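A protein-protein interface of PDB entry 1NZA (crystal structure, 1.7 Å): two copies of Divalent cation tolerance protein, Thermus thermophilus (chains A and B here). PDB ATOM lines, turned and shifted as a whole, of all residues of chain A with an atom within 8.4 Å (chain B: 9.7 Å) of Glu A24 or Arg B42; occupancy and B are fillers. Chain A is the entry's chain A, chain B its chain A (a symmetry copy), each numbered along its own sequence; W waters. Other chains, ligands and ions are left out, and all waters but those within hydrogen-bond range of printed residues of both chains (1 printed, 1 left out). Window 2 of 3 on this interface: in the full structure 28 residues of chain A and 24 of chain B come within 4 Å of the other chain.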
ATOM      1  N   ARG A  16       1.863  -8.353   9.305  1.00  0.00           N
ATOM      2  CA  ARG A  16       1.334  -9.201   8.245  1.00  0.00           C
ATOM      3  C   ARG A  16      -0.150  -8.976   7.967  1.00  0.00           C
ATOM      4  O   ARG A  16      -0.571  -8.949   6.808  1.00  0.00           O
ATOM      5  CB  ARG A  16       1.586 -10.672   8.589  1.00  0.00           C
ATOM      6  CG  ARG A  16       3.061 -11.030   8.622  1.00  0.00           C
ATOM      7  CD  ARG A  16       3.255 -12.508   8.905  1.00  0.00           C
ATOM      8  NE  ARG A  16       2.705 -13.336   7.831  1.00  0.00           N
ATOM      9  CZ  ARG A  16       3.282 -13.509   6.647  1.00  0.00           C
ATOM     10  NH1 ARG A  16       2.701 -14.277   5.732  1.00  0.00           N
ATOM     11  NH2 ARG A  16       4.445 -12.928   6.377  1.00  0.00           N
ATOM     12  N   THR A  17      -0.935  -8.820   9.028  1.00  0.00           N
ATOM     13  CA  THR A  17      -2.370  -8.586   8.884  1.00  0.00           C
ATOM     14  C   THR A  17      -2.612  -7.309   8.078  1.00  0.00           C
ATOM     15  O   THR A  17      -3.416  -7.292   7.137  1.00  0.00           O
ATOM     16  CB  THR A  17      -3.044  -8.437  10.254  1.00  0.00           C
ATOM     17  OG1 THR A  17      -2.833  -9.628  11.020  1.00  0.00           O
ATOM     18  CG2 THR A  17      -4.540  -8.193  10.092  1.00  0.00           C
ATOM     19  N   ILE A  18      -1.914  -6.236   8.442  1.00  0.00           N
ATOM     20  CA  ILE A  18      -2.075  -4.977   7.719  1.00  0.00           C
ATOM     21  C   ILE A  18      -1.544  -5.069   6.291  1.00  0.00           C
ATOM     22  O   ILE A  18      -2.185  -4.594   5.347  1.00  0.00           O
ATOM     23  CB  ILE A  18      -1.392  -3.817   8.475  1.00  0.00           C
ATOM     24  CG1 ILE A  18      -2.204  -3.481   9.727  1.00  0.00           C
ATOM     25  CG2 ILE A  18      -1.270  -2.591   7.582  1.00  0.00           C
ATOM     26  CD1 ILE A  18      -1.556  -2.439  10.615  1.00  0.00           C
ATOM     27  N   ALA A  19      -0.381  -5.688   6.116  1.00  0.00           N
ATOM     28  CA  ALA A  19       0.179  -5.822   4.775  1.00  0.00           C
ATOM     29  C   ALA A  19      -0.777  -6.593   3.871  1.00  0.00           C
ATOM     30  O   ALA A  19      -1.051  -6.179   2.746  1.00  0.00           O
ATOM     31  CB  ALA A  19       1.534  -6.533   4.831  1.00  0.00           C
ATOM     32  N   LYS A  20      -1.295  -7.714   4.369  1.00  0.00           N
ATOM     33  CA  LYS A  20      -2.206  -8.525   3.573  1.00  0.00           C
ATOM     34  C   LYS A  20      -3.513  -7.801   3.288  1.00  0.00           C
ATOM     35  O   LYS A  20      -4.003  -7.810   2.158  1.00  0.00           O
ATOM     36  CB  LYS A  20      -2.488  -9.857   4.274  1.00  0.00           C
ATOM     37  CG  LYS A  20      -1.287 -10.782   4.327  1.00  0.00           C
ATOM     38  CD  LYS A  20      -1.689 -12.194   4.728  1.00  0.00           C
ATOM     39  CE  LYS A  20      -2.296 -12.239   6.118  1.00  0.00           C
ATOM     40  NZ  LYS A  20      -2.642 -13.635   6.508  1.00  0.00           N
ATOM     41  N   ALA A  21      -4.074  -7.168   4.310  1.00  0.00           N
ATOM     42  CA  ALA A  21      -5.331  -6.445   4.153  1.00  0.00           C
ATOM     43  C   ALA A  21      -5.223  -5.345   3.098  1.00  0.00           C
ATOM     44  O   ALA A  21      -6.098  -5.210   2.245  1.00  0.00           O
ATOM     45  CB  ALA A  21      -5.760  -5.857   5.485  1.00  0.00           C
ATOM     46  N   LEU A  22      -4.146  -4.567   3.140  1.00  0.00           N
ATOM     47  CA  LEU A  22      -3.971  -3.492   2.169  1.00  0.00           C
ATOM     48  C   LEU A  22      -3.818  -4.002   0.735  1.00  0.00           C
ATOM     49  O   LEU A  22      -4.416  -3.450  -0.196  1.00  0.00           O
ATOM     50  CB  LEU A  22      -2.767  -2.626   2.558  1.00  0.00           C
ATOM     51  CG  LEU A  22      -2.977  -1.871   3.870  1.00  0.00           C
ATOM     52  CD1 LEU A  22      -1.727  -1.098   4.245  1.00  0.00           C
ATOM     53  CD2 LEU A  22      -4.170  -0.930   3.714  1.00  0.00           C
ATOM     54  N   VAL A  23      -3.034  -5.057   0.544  1.00  0.00           N
ATOM     55  CA  VAL A  23      -2.846  -5.591  -0.796  1.00  0.00           C
ATOM     56  C   VAL A  23      -4.105  -6.308  -1.289  1.00  0.00           C
ATOM     57  O   VAL A  23      -4.511  -6.137  -2.441  1.00  0.00           O
ATOM     58  CB  VAL A  23      -1.642  -6.558  -0.855  1.00  0.00           C
ATOM     59  CG1 VAL A  23      -1.454  -7.072  -2.273  1.00  0.00           C
ATOM     60  CG2 VAL A  23      -0.378  -5.834  -0.391  1.00  0.00           C
ATOM     61  N   GLU A  24      -4.725  -7.102  -0.421  1.00  0.00           N
ATOM     62  CA  GLU A  24      -5.942  -7.823  -0.797  1.00  0.00           C
ATOM     63  C   GLU A  24      -7.010  -6.837  -1.266  1.00  0.00           C
ATOM     64  O   GLU A  24      -7.660  -7.044  -2.290  1.00  0.00           O
ATOM     65  CB  GLU A  24      -6.508  -8.611   0.393  1.00  0.00           C
ATOM     66  CG  GLU A  24      -5.614  -9.703   0.953  1.00  0.00           C
ATOM     67  CD  GLU A  24      -6.267 -10.450   2.109  1.00  0.00           C
ATOM     68  OE1 GLU A  24      -6.845  -9.791   3.005  1.00  0.00           O
ATOM     69  OE2 GLU A  24      -6.196 -11.699   2.128  1.00  0.00           O
ATOM     70  N   GLU A  25      -7.177  -5.764  -0.501  1.00  0.00           N
ATOM     71  CA  GLU A  25      -8.180  -4.747  -0.789  1.00  0.00           C
ATOM     72  C   GLU A  25      -7.768  -3.719  -1.833  1.00  0.00           C
ATOM     73  O   GLU A  25      -8.408  -2.675  -1.972  1.00  0.00           O
ATOM     74  CB  GLU A  25      -8.570  -4.047   0.511  1.00  0.00           C
ATOM     75  CG  GLU A  25      -9.302  -4.963   1.479  1.00  0.00           C
ATOM     76  CD  GLU A  25      -9.549  -4.322   2.829  1.00  0.00           C
ATOM     77  OE1 GLU A  25      -9.988  -3.154   2.867  1.00  0.00           O
ATOM     78  OE2 GLU A  25      -9.312  -4.995   3.856  1.00  0.00           O
ATOM     79  N   ARG A  26      -6.707  -4.025  -2.569  1.00  0.00           N
ATOM     80  CA  ARG A  26      -6.197  -3.146  -3.617  1.00  0.00           C
ATOM     81  C   ARG A  26      -5.962  -1.705  -3.169  1.00  0.00           C
ATOM     82  O   ARG A  26      -6.184  -0.765  -3.934  1.00  0.00           O
ATOM     83  CB  ARG A  26      -7.138  -3.160  -4.828  1.00  0.00           C
ATOM     84  CG  ARG A  26      -7.419  -4.547  -5.393  1.00  0.00           C
ATOM     85  CD  ARG A  26      -8.175  -4.459  -6.715  1.00  0.00           C
ATOM     86  NE  ARG A  26      -7.282  -4.202  -7.842  1.00  0.00           N
ATOM     87  CZ  ARG A  26      -6.643  -5.152  -8.520  1.00  0.00           C
ATOM     88  NH1 ARG A  26      -6.800  -6.428  -8.191  1.00  0.00           N
ATOM     89  NH2 ARG A  26      -5.838  -4.827  -9.524  1.00  0.00           N
ATOM     90  N   LEU A  27      -5.520  -1.529  -1.929  1.00  0.00           N
ATOM     91  CA  LEU A  27      -5.230  -0.193  -1.421  1.00  0.00           C
ATOM     92  C   LEU A  27      -3.727   0.030  -1.529  1.00  0.00           C
ATOM     93  O   LEU A  27      -3.214   1.109  -1.224  1.00  0.00           O
ATOM     94  CB  LEU A  27      -5.689  -0.052   0.030  1.00  0.00           C
ATOM     95  CG  LEU A  27      -7.206  -0.096   0.243  1.00  0.00           C
ATOM     96  CD1 LEU A  27      -7.514   0.055   1.717  1.00  0.00           C
ATOM     97  CD2 LEU A  27      -7.872   1.016  -0.566  1.00  0.00           C
ATOM     98  N   ALA A  28      -3.035  -1.013  -1.970  1.00  0.00           N
ATOM     99  CA  ALA A  28      -1.590  -0.982  -2.151  1.00  0.00           C
ATOM    100  C   ALA A  28      -1.258  -2.152  -3.070  1.00  0.00           C
ATOM    101  O   ALA A  28      -1.951  -3.171  -3.054  1.00  0.00           O
ATOM    102  CB  ALA A  28      -0.885  -1.134  -0.810  1.00  0.00           C
ATOM    103  N   ALA A  29      -0.215  -2.003  -3.879  1.00  0.00           N
ATOM    104  CA  ALA A  29       0.179  -3.054  -4.806  1.00  0.00           C
ATOM    105  C   ALA A  29       1.262  -3.920  -4.186  1.00  0.00           C
ATOM    106  O   ALA A  29       1.396  -5.102  -4.506  1.00  0.00           O
ATOM    107  CB  ALA A  29       0.699  -2.446  -6.095  1.00  0.00           C
ATOM    108  N   CYS A  30       2.034  -3.317  -3.291  1.00  0.00           N
ATOM    109  CA  CYS A  30       3.127  -4.026  -2.642  1.00  0.00           C
ATOM    110  C   CYS A  30       3.371  -3.480  -1.249  1.00  0.00           C
ATOM    111  O   CYS A  30       3.169  -2.292  -0.995  1.00  0.00           O
ATOM    112  CB  CYS A  30       4.394  -3.863  -3.480  1.00  0.00           C
ATOM    113  SG  CYS A  30       5.882  -4.601  -2.769  1.00  0.00           S
ATOM    114  N   VAL A  31       3.797  -4.350  -0.341  1.00  0.00           N
ATOM    115  CA  VAL A  31       4.113  -3.923   1.016  1.00  0.00           C
ATOM    116  C   VAL A  31       5.358  -4.668   1.472  1.00  0.00           C
ATOM    117  O   VAL A  31       5.414  -5.896   1.377  1.00  0.00           O
ATOM    118  CB  VAL A  31       2.973  -4.237   2.006  1.00  0.00           C
ATOM    119  CG1 VAL A  31       3.402  -3.871   3.415  1.00  0.00           C
ATOM    120  CG2 VAL A  31       1.716  -3.459   1.631  1.00  0.00           C
ATOM    121  N   ARG A  70      -8.503   1.986   6.777  1.00  0.00           N
ATOM    122  CA  ARG A  70      -8.278   0.571   7.027  1.00  0.00           C
ATOM    123  C   ARG A  70      -7.156   0.368   8.044  1.00  0.00           C
ATOM    124  O   ARG A  70      -7.252  -0.494   8.914  1.00  0.00           O
ATOM    125  CB  ARG A  70      -7.950  -0.153   5.718  1.00  0.00           C
ATOM    126  CG  ARG A  70      -9.021  -0.002   4.641  1.00  0.00           C
ATOM    127  CD  ARG A  70     -10.363  -0.614   5.054  1.00  0.00           C
ATOM    128  NE  ARG A  70     -10.308  -2.073   5.134  1.00  0.00           N
ATOM    129  CZ  ARG A  70     -10.495  -2.771   6.250  1.00  0.00           C
ATOM    130  NH1 ARG A  70     -10.750  -2.146   7.395  1.00  0.00           N
ATOM    131  NH2 ARG A  70     -10.431  -4.097   6.223  1.00  0.00           N
ATOM    132  N   LEU A  74      -7.367  -1.649  11.682  1.00  0.00           N
ATOM    133  CA  LEU A  74      -6.557  -2.828  11.970  1.00  0.00           C
ATOM    134  C   LEU A  74      -5.476  -2.576  13.018  1.00  0.00           C
ATOM    135  O   LEU A  74      -5.203  -3.439  13.848  1.00  0.00           O
ATOM    136  CB  LEU A  74      -5.907  -3.340  10.681  1.00  0.00           C
ATOM    137  CG  LEU A  74      -6.837  -3.848   9.573  1.00  0.00           C
ATOM    138  CD1 LEU A  74      -6.042  -4.082   8.303  1.00  0.00           C
ATOM    139  CD2 LEU A  74      -7.527  -5.133  10.018  1.00  0.00           C
ATOM    140  N   TRP A  97       2.322  -0.752 -13.019  1.00  0.00           N
ATOM    141  CA  TRP A  97       1.838  -1.934 -12.314  1.00  0.00           C
ATOM    142  C   TRP A  97       1.280  -1.489 -10.969  1.00  0.00           C
ATOM    143  O   TRP A  97       0.269  -2.007 -10.495  1.00  0.00           O
ATOM    144  CB  TRP A  97       2.992  -2.921 -12.086  1.00  0.00           C
ATOM    145  CG  TRP A  97       2.676  -4.012 -11.093  1.00  0.00           C
ATOM    146  CD1 TRP A  97       1.930  -5.138 -11.312  1.00  0.00           C
ATOM    147  CD2 TRP A  97       3.063  -4.050  -9.713  1.00  0.00           C
ATOM    148  NE1 TRP A  97       1.828  -5.872 -10.153  1.00  0.00           N
ATOM    149  CE2 TRP A  97       2.514  -5.227  -9.156  1.00  0.00           C
ATOM    150  CE3 TRP A  97       3.822  -3.202  -8.892  1.00  0.00           C
ATOM    151  CZ2 TRP A  97       2.698  -5.580  -7.812  1.00  0.00           C
ATOM    152  CZ3 TRP A  97       4.007  -3.553  -7.555  1.00  0.00           C
ATOM    153  CH2 TRP A  97       3.444  -4.733  -7.031  1.00  0.00           C
ATOM    154  N   LEU A  98       1.951  -0.516 -10.363  1.00  0.00           N
ATOM    155  CA  LEU A  98       1.549   0.014  -9.068  1.00  0.00           C
ATOM    156  C   LEU A  98       0.165   0.657  -9.151  1.00  0.00           C
ATOM    157  O   LEU A  98      -0.701   0.385  -8.322  1.00  0.00           O
ATOM    158  CB  LEU A  98       2.591   1.030  -8.583  1.00  0.00           C
ATOM    159  CG  LEU A  98       2.517   1.557  -7.147  1.00  0.00           C
ATOM    160  CD1 LEU A  98       3.793   2.323  -6.830  1.00  0.00           C
ATOM    161  CD2 LEU A  98       1.298   2.456  -6.969  1.00  0.00           C
ATOM    162  N   GLU A 100      -2.034   0.321 -11.706  1.00  0.00           N
ATOM    163  CA  GLU A 100      -2.917  -0.715 -12.229  1.00  0.00           C
ATOM    164  C   GLU A 100      -3.494  -1.624 -11.142  1.00  0.00           C
ATOM    165  O   GLU A 100      -4.611  -2.124 -11.275  1.00  0.00           O
ATOM    166  CB  GLU A 100      -2.151  -1.558 -13.256  1.00  0.00           C
ATOM    167  CG  GLU A 100      -2.785  -2.900 -13.603  1.00  0.00           C
ATOM    168  CD  GLU A 100      -1.965  -3.689 -14.613  1.00  0.00           C
ATOM    169  OE1 GLU A 100      -1.900  -3.270 -15.789  1.00  0.00           O
ATOM    170  OE2 GLU A 100      -1.377  -4.725 -14.232  1.00  0.00           O
ATOM    171  N   ASN A 101      -2.738  -1.831 -10.067  1.00  0.00           N
ATOM    172  CA  ASN A 101      -3.182  -2.705  -8.982  1.00  0.00           C
ATOM    173  C   ASN A 101      -3.615  -1.990  -7.706  1.00  0.00           C
ATOM    174  O   ASN A 101      -3.746  -2.613  -6.652  1.00  0.00           O
ATOM    175  CB  ASN A 101      -2.079  -3.716  -8.659  1.00  0.00           C
ATOM    176  CG  ASN A 101      -1.850  -4.699  -9.786  1.00  0.00           C
ATOM    177  OD1 ASN A 101      -2.686  -5.561 -10.052  1.00  0.00           O
ATOM    178  ND2 ASN A 101      -0.720  -4.569 -10.464  1.00  0.00           N
ATOM    179  N   THR A 102      -3.839  -0.684  -7.800  1.00  0.00           N
ATOM    180  CA  THR A 102      -4.275   0.097  -6.652  1.00  0.00           C
ATOM    181  C   THR A 102      -5.602   0.768  -6.994  1.00  0.00           C
ATOM    182  O   THR A 102      -5.790   1.248  -8.110  1.00  0.00           O
ATOM    183  CB  THR A 102      -3.228   1.177  -6.278  1.00  0.00           C
ATOM    184  OG1 THR A 102      -1.993   0.540  -5.927  1.00  0.00           O
ATOM    185  CG2 THR A 102      -3.709   2.003  -5.097  1.00  0.00           C
ATOM    186  N   GLY A 103      -6.525   0.789  -6.038  1.00  0.00           N
ATOM    187  CA  GLY A 103      -7.817   1.406  -6.282  1.00  0.00           C
ATOM    188  C   GLY A 103      -8.130   2.528  -5.310  1.00  0.00           C
ATOM    189  O   GLY A 103      -8.137   3.701  -5.740  1.00  0.00           O
ATOM    190  OXT GLY A 103      -8.364   2.238  -4.117  1.00  0.00           O
ATOM    191  N   SER B  39       8.088  -9.449   1.608  1.00  0.00           N
ATOM    192  CA  SER B  39       7.330  -8.617   0.687  1.00  0.00           C
ATOM    193  C   SER B  39       6.026  -9.296   0.304  1.00  0.00           C
ATOM    194  O   SER B  39       5.995 -10.482  -0.029  1.00  0.00           O
ATOM    195  CB  SER B  39       8.166  -8.310  -0.552  1.00  0.00           C
ATOM    196  OG  SER B  39       9.352  -7.622  -0.180  1.00  0.00           O
ATOM    197  N   ILE B  40       4.942  -8.531   0.374  1.00  0.00           N
ATOM    198  CA  ILE B  40       3.620  -9.044   0.046  1.00  0.00           C
ATOM    199  C   ILE B  40       3.057  -8.151  -1.055  1.00  0.00           C
ATOM    200  O   ILE B  40       2.861  -6.952  -0.852  1.00  0.00           O
ATOM    201  CB  ILE B  40       2.707  -9.023   1.298  1.00  0.00           C
ATOM    202  CG1 ILE B  40       3.327  -9.905   2.394  1.00  0.00           C
ATOM    203  CG2 ILE B  40       1.319  -9.534   0.952  1.00  0.00           C
ATOM    204  CD1 ILE B  40       2.560  -9.920   3.699  1.00  0.00           C
ATOM    205  N   TYR B  41       2.820  -8.733  -2.226  1.00  0.00           N
ATOM    206  CA  TYR B  41       2.306  -7.961  -3.349  1.00  0.00           C
ATOM    207  C   TYR B  41       1.275  -8.696  -4.189  1.00  0.00           C
ATOM    208  O   TYR B  41       1.082  -9.900  -4.051  1.00  0.00           O
ATOM    209  CB  TYR B  41       3.460  -7.505  -4.247  1.00  0.00           C
ATOM    210  CG  TYR B  41       4.411  -8.602  -4.665  1.00  0.00           C
ATOM    211  CD1 TYR B  41       5.359  -9.115  -3.773  1.00  0.00           C
ATOM    212  CD2 TYR B  41       4.373  -9.124  -5.956  1.00  0.00           C
ATOM    213  CE1 TYR B  41       6.246 -10.118  -4.161  1.00  0.00           C
ATOM    214  CE2 TYR B  41       5.253 -10.126  -6.358  1.00  0.00           C
ATOM    215  CZ  TYR B  41       6.188 -10.619  -5.455  1.00  0.00           C
ATOM    216  OH  TYR B  41       7.058 -11.608  -5.849  1.00  0.00           O
ATOM    217  N   ARG B  42       0.611  -7.957  -5.067  1.00  0.00           N
ATOM    218  CA  ARG B  42      -0.399  -8.554  -5.926  1.00  0.00           C
ATOM    219  C   ARG B  42       0.194  -9.023  -7.244  1.00  0.00           C
ATOM    220  O   ARG B  42       0.999  -8.330  -7.865  1.00  0.00           O
ATOM    221  CB  ARG B  42      -1.521  -7.554  -6.198  1.00  0.00           C
ATOM    222  CG  ARG B  42      -2.555  -8.053  -7.186  1.00  0.00           C
ATOM    223  CD  ARG B  42      -3.763  -7.146  -7.199  1.00  0.00           C
ATOM    224  NE  ARG B  42      -4.463  -7.175  -5.918  1.00  0.00           N
ATOM    225  CZ  ARG B  42      -5.075  -8.246  -5.425  1.00  0.00           C
ATOM    226  NH1 ARG B  42      -5.080  -9.385  -6.103  1.00  0.00           N
ATOM    227  NH2 ARG B  42      -5.680  -8.181  -4.246  1.00  0.00           N
ATOM    228  N   TRP B  43      -0.215 -10.214  -7.663  1.00  0.00           N
ATOM    229  CA  TRP B  43       0.256 -10.790  -8.910  1.00  0.00           C
ATOM    230  C   TRP B  43      -0.832 -11.711  -9.455  1.00  0.00           C
ATOM    231  O   TRP B  43      -1.138 -12.748  -8.865  1.00  0.00           O
ATOM    232  CB  TRP B  43       1.546 -11.574  -8.670  1.00  0.00           C
ATOM    233  CG  TRP B  43       2.317 -11.851  -9.917  1.00  0.00           C
ATOM    234  CD1 TRP B  43       2.719 -10.939 -10.851  1.00  0.00           C
ATOM    235  CD2 TRP B  43       2.818 -13.120 -10.355  1.00  0.00           C
ATOM    236  NE1 TRP B  43       3.440 -11.561 -11.843  1.00  0.00           N
ATOM    237  CE2 TRP B  43       3.516 -12.901 -11.563  1.00  0.00           C
ATOM    238  CE3 TRP B  43       2.745 -14.423  -9.841  1.00  0.00           C
ATOM    239  CZ2 TRP B  43       4.140 -13.935 -12.269  1.00  0.00           C
ATOM    240  CZ3 TRP B  43       3.367 -15.453 -10.543  1.00  0.00           C
ATOM    241  CH2 TRP B  43       4.055 -15.201 -11.745  1.00  0.00           C
ATOM    242  N   GLN B  44      -1.429 -11.311 -10.573  1.00  0.00           N
ATOM    243  CA  GLN B  44      -2.491 -12.094 -11.194  1.00  0.00           C
ATOM    244  C   GLN B  44      -3.679 -12.203 -10.244  1.00  0.00           C
ATOM    245  O   GLN B  44      -4.194 -13.297 -10.004  1.00  0.00           O
ATOM    246  CB  GLN B  44      -1.981 -13.496 -11.535  1.00  0.00           C
ATOM    247  CG  GLN B  44      -0.670 -13.514 -12.304  1.00  0.00           C
ATOM    248  CD  GLN B  44      -0.786 -12.899 -13.686  1.00  0.00           C
ATOM    249  OE1 GLN B  44       0.203 -12.797 -14.416  1.00  0.00           O
ATOM    250  NE2 GLN B  44      -1.995 -12.490 -14.055  1.00  0.00           N
ATOM    251  N   GLY B  45      -4.109 -11.068  -9.702  1.00  0.00           N
ATOM    252  CA  GLY B  45      -5.232 -11.076  -8.781  1.00  0.00           C
ATOM    253  C   GLY B  45      -5.012 -12.069  -7.656  1.00  0.00           C
ATOM    254  O   GLY B  45      -5.953 -12.694  -7.164  1.00  0.00           O
ATOM    255  N   GLU B  46      -3.755 -12.212  -7.252  1.00  0.00           N
ATOM    256  CA  GLU B  46      -3.379 -13.131  -6.187  1.00  0.00           C
ATOM    257  C   GLU B  46      -2.318 -12.470  -5.312  1.00  0.00           C
ATOM    258  O   GLU B  46      -1.326 -11.951  -5.821  1.00  0.00           O
ATOM    259  CB  GLU B  46      -2.818 -14.419  -6.795  1.00  0.00           C
ATOM    260  CG  GLU B  46      -2.508 -15.513  -5.793  1.00  0.00           C
ATOM    261  CD  GLU B  46      -1.856 -16.720  -6.445  1.00  0.00           C
ATOM    262  OE1 GLU B  46      -2.431 -17.256  -7.418  1.00  0.00           O
ATOM    263  OE2 GLU B  46      -0.771 -17.134  -5.984  1.00  0.00           O
ATOM    264  N   VAL B  47      -2.535 -12.482  -4.002  1.00  0.00           N
ATOM    265  CA  VAL B  47      -1.587 -11.889  -3.063  1.00  0.00           C
ATOM    266  C   VAL B  47      -0.475 -12.899  -2.774  1.00  0.00           C
ATOM    267  O   VAL B  47      -0.725 -13.936  -2.154  1.00  0.00           O
ATOM    268  CB  VAL B  47      -2.290 -11.508  -1.740  1.00  0.00           C
ATOM    269  CG1 VAL B  47      -1.304 -10.853  -0.791  1.00  0.00           C
ATOM    270  CG2 VAL B  47      -3.453 -10.569  -2.023  1.00  0.00           C
ATOM    271  N   VAL B  48       0.742 -12.598  -3.229  1.00  0.00           N
ATOM    272  CA  VAL B  48       1.882 -13.492  -3.026  1.00  0.00           C
ATOM    273  C   VAL B  48       2.924 -12.911  -2.075  1.00  0.00           C
ATOM    274  O   VAL B  48       2.895 -11.724  -1.754  1.00  0.00           O
ATOM    275  CB  VAL B  48       2.571 -13.832  -4.361  1.00  0.00           C
ATOM    276  CG1 VAL B  48       1.584 -14.531  -5.281  1.00  0.00           C
ATOM    277  CG2 VAL B  48       3.107 -12.568  -5.009  1.00  0.00           C
ATOM    278  N   GLU B  49       3.856 -13.755  -1.646  1.00  0.00           N
ATOM    279  CA  GLU B  49       4.888 -13.335  -0.704  1.00  0.00           C
ATOM    280  C   GLU B  49       6.285 -13.684  -1.192  1.00  0.00           C
ATOM    281  O   GLU B  49       6.469 -14.641  -1.941  1.00  0.00           O
ATOM    282  CB  GLU B  49       4.625 -14.009   0.642  1.00  0.00           C
ATOM    283  CG  GLU B  49       5.476 -13.514   1.783  1.00  0.00           C
ATOM    284  CD  GLU B  49       4.981 -14.041   3.109  1.00  0.00           C
ATOM    285  OE1 GLU B  49       3.751 -14.013   3.330  1.00  0.00           O
ATOM    286  OE2 GLU B  49       5.814 -14.476   3.929  1.00  0.00           O
ATOM    287  N   ASP B  50       7.276 -12.910  -0.761  1.00  0.00           N
ATOM    288  CA  ASP B  50       8.646 -13.162  -1.165  1.00  0.00           C
ATOM    289  C   ASP B  50       9.606 -12.673  -0.083  1.00  0.00           C
ATOM    290  O   ASP B  50       9.224 -11.884   0.774  1.00  0.00           O
ATOM    291  CB  ASP B  50       8.927 -12.441  -2.488  1.00  0.00           C
ATOM    292  CG  ASP B  50      10.184 -12.920  -3.149  1.00  0.00           C
ATOM    293  OD1 ASP B  50      10.684 -13.974  -2.723  1.00  0.00           O
ATOM    294  OD2 ASP B  50      10.667 -12.269  -4.098  1.00  0.00           O
HETATM  295  O   HOH W   1      -7.655 -10.303  -3.229  1.00  0.00           O
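No position is printed for both chains.
Of the 12 printed residues of chain B, 6 touch a printed residue of chain A.
Hydrophobic or aromatic side chains of chain B within 4 Å of the printed part of chain A: Ile B40, Tyr B41 and Val B47.
Of the 24 printed residues of chain A, 11 touch a printed residue of chain B.
Hydrophobic or aromatic side chains of chain A that line the printed part of chain B: Ala A19, Val A23, Val A31 and Trp A97.
Among the printed residues, 18 pairs touch across the chains.
Among the printed residues, Asp or Glu carboxylates within 4 Å of a Lys or Arg side-chain nitrogen of the other chain: Arg A16 with Glu B49.
CB of Ala A19 touches CD1 of Ile B40, at 3.7 Å.
CD1 of Ile B40 touches CG of Lys A20, at 3.99 Å.
Ile B40 touches Val A23.
CG1 of Val A23 touches C of Tyr B41, at 3.7 Å.
Val B47 touches Glu A24.
Cys A30 touches Ile B40 (CA to O, 3.4 Å).
Cys A30 touches Tyr B41 (CB to CB, 3.8 Å).
Val A31 touches Ser B39.
CH2 of Trp A97 touches CB of Tyr B41 (3.9 Å).
Asn A101 touches Arg B42 (OD1 to CD, 3.4 Å).
The guanidinium group (NH2) of Arg A26 sits at hydrogen-bond distance from the backbone carbonyl oxygen (O) of Glu A100 (3.4 Å).
OD1 of Asn A101 sits at hydrogen-bond distance from NH2 of Arg A26.
The backbone carbonyl oxygen (O) of Arg A26 lies within hydrogen-bond range of the backbone NH (N) of Gly A103.
The backbone carbonyl oxygen of Trp A97 lies within hydrogen-bond range of the side-chain amide nitrogen of Asn A101 (2.7 Å).
O of Asp B50 sits at hydrogen-bond distance from N of Ser B39.
The backbone carbonyl oxygen (O) of Tyr B41 sits at hydrogen-bond distance from the backbone NH (N) of Val B48, at 2.8 Å.
Water W1 bridges the guanidinium group (NH2) of Arg B42 (3.1 Å) and the backbone carbonyl oxygen (O) of Glu A24 (3.4 Å).
Of the printed residues of chain B, Arg A16 touches Glu B49 (2.6 Å).
Printed residues of chain B within 4 Å of Ala A19: Ile B40 (3.7 Å).
No residue of chain B comes within 4 Å of Ala A21.
Val A23 touches three residues of chain B.
Of chain B, only Arg B42 (3.0 Å) and Val B47 (3.8 Å) come within 4 Å of Glu A24.
Printed residues of chain B within 4 Å of Ala A29: Tyr B41 and Arg B42.
Of the printed residues of chain B, Trp A97 touches Tyr B41 and Arg B42.
Of the printed residues of chain A, Arg B42 touches Val A23 (3.0 Å), Glu A24 (3.0 Å), Arg A26 (3.3 Å), Ala A29 (3.0 Å), Trp A97 (3.2 Å) and Asn A101 (3.4 Å).
No residue of chain A comes within 4 Å of Gly B45.
The nearest residue of chain B that does not touch Glu A24 is Ile B40 (6.7 Å).
The nearest residue of chain A that does not touch Arg B42 is Glu A25 (4.7 Å).
The nearest printed residue of chain A that does not touch Ser B39 is Cys A30 (4.9 Å).
The side-chain carboxylate (OE1) of Glu B49 lies within salt-bridge range of the guanidinium group (NH1) of Arg A16.
The guanidinium group (NH2) of Arg B42 lies within hydrogen-bond range of the backbone carbonyl oxygen (O) of Val A23, 3.0 Å away.
The backbone carbonyl oxygen (O) of Glu A24 lies within hydrogen-bond range of the guanidinium group (NH2) of Arg B42 (3.0 Å).
The backbone carbonyl oxygen (O) of Ala A29 lies within hydrogen-bond range of the backbone NH (N) of Arg B42, at 3.0 Å.
The backbone NH of Val A31 sits at hydrogen-bond distance from the backbone carbonyl oxygen of Ile B40.
NE1 of Trp A97 sits close to O of Arg B42 (3.5 Å).
The guanidinium group (NH1) of Arg A26 lies close to the guanidinium group (NE) of Arg B42 (3.3 Å).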
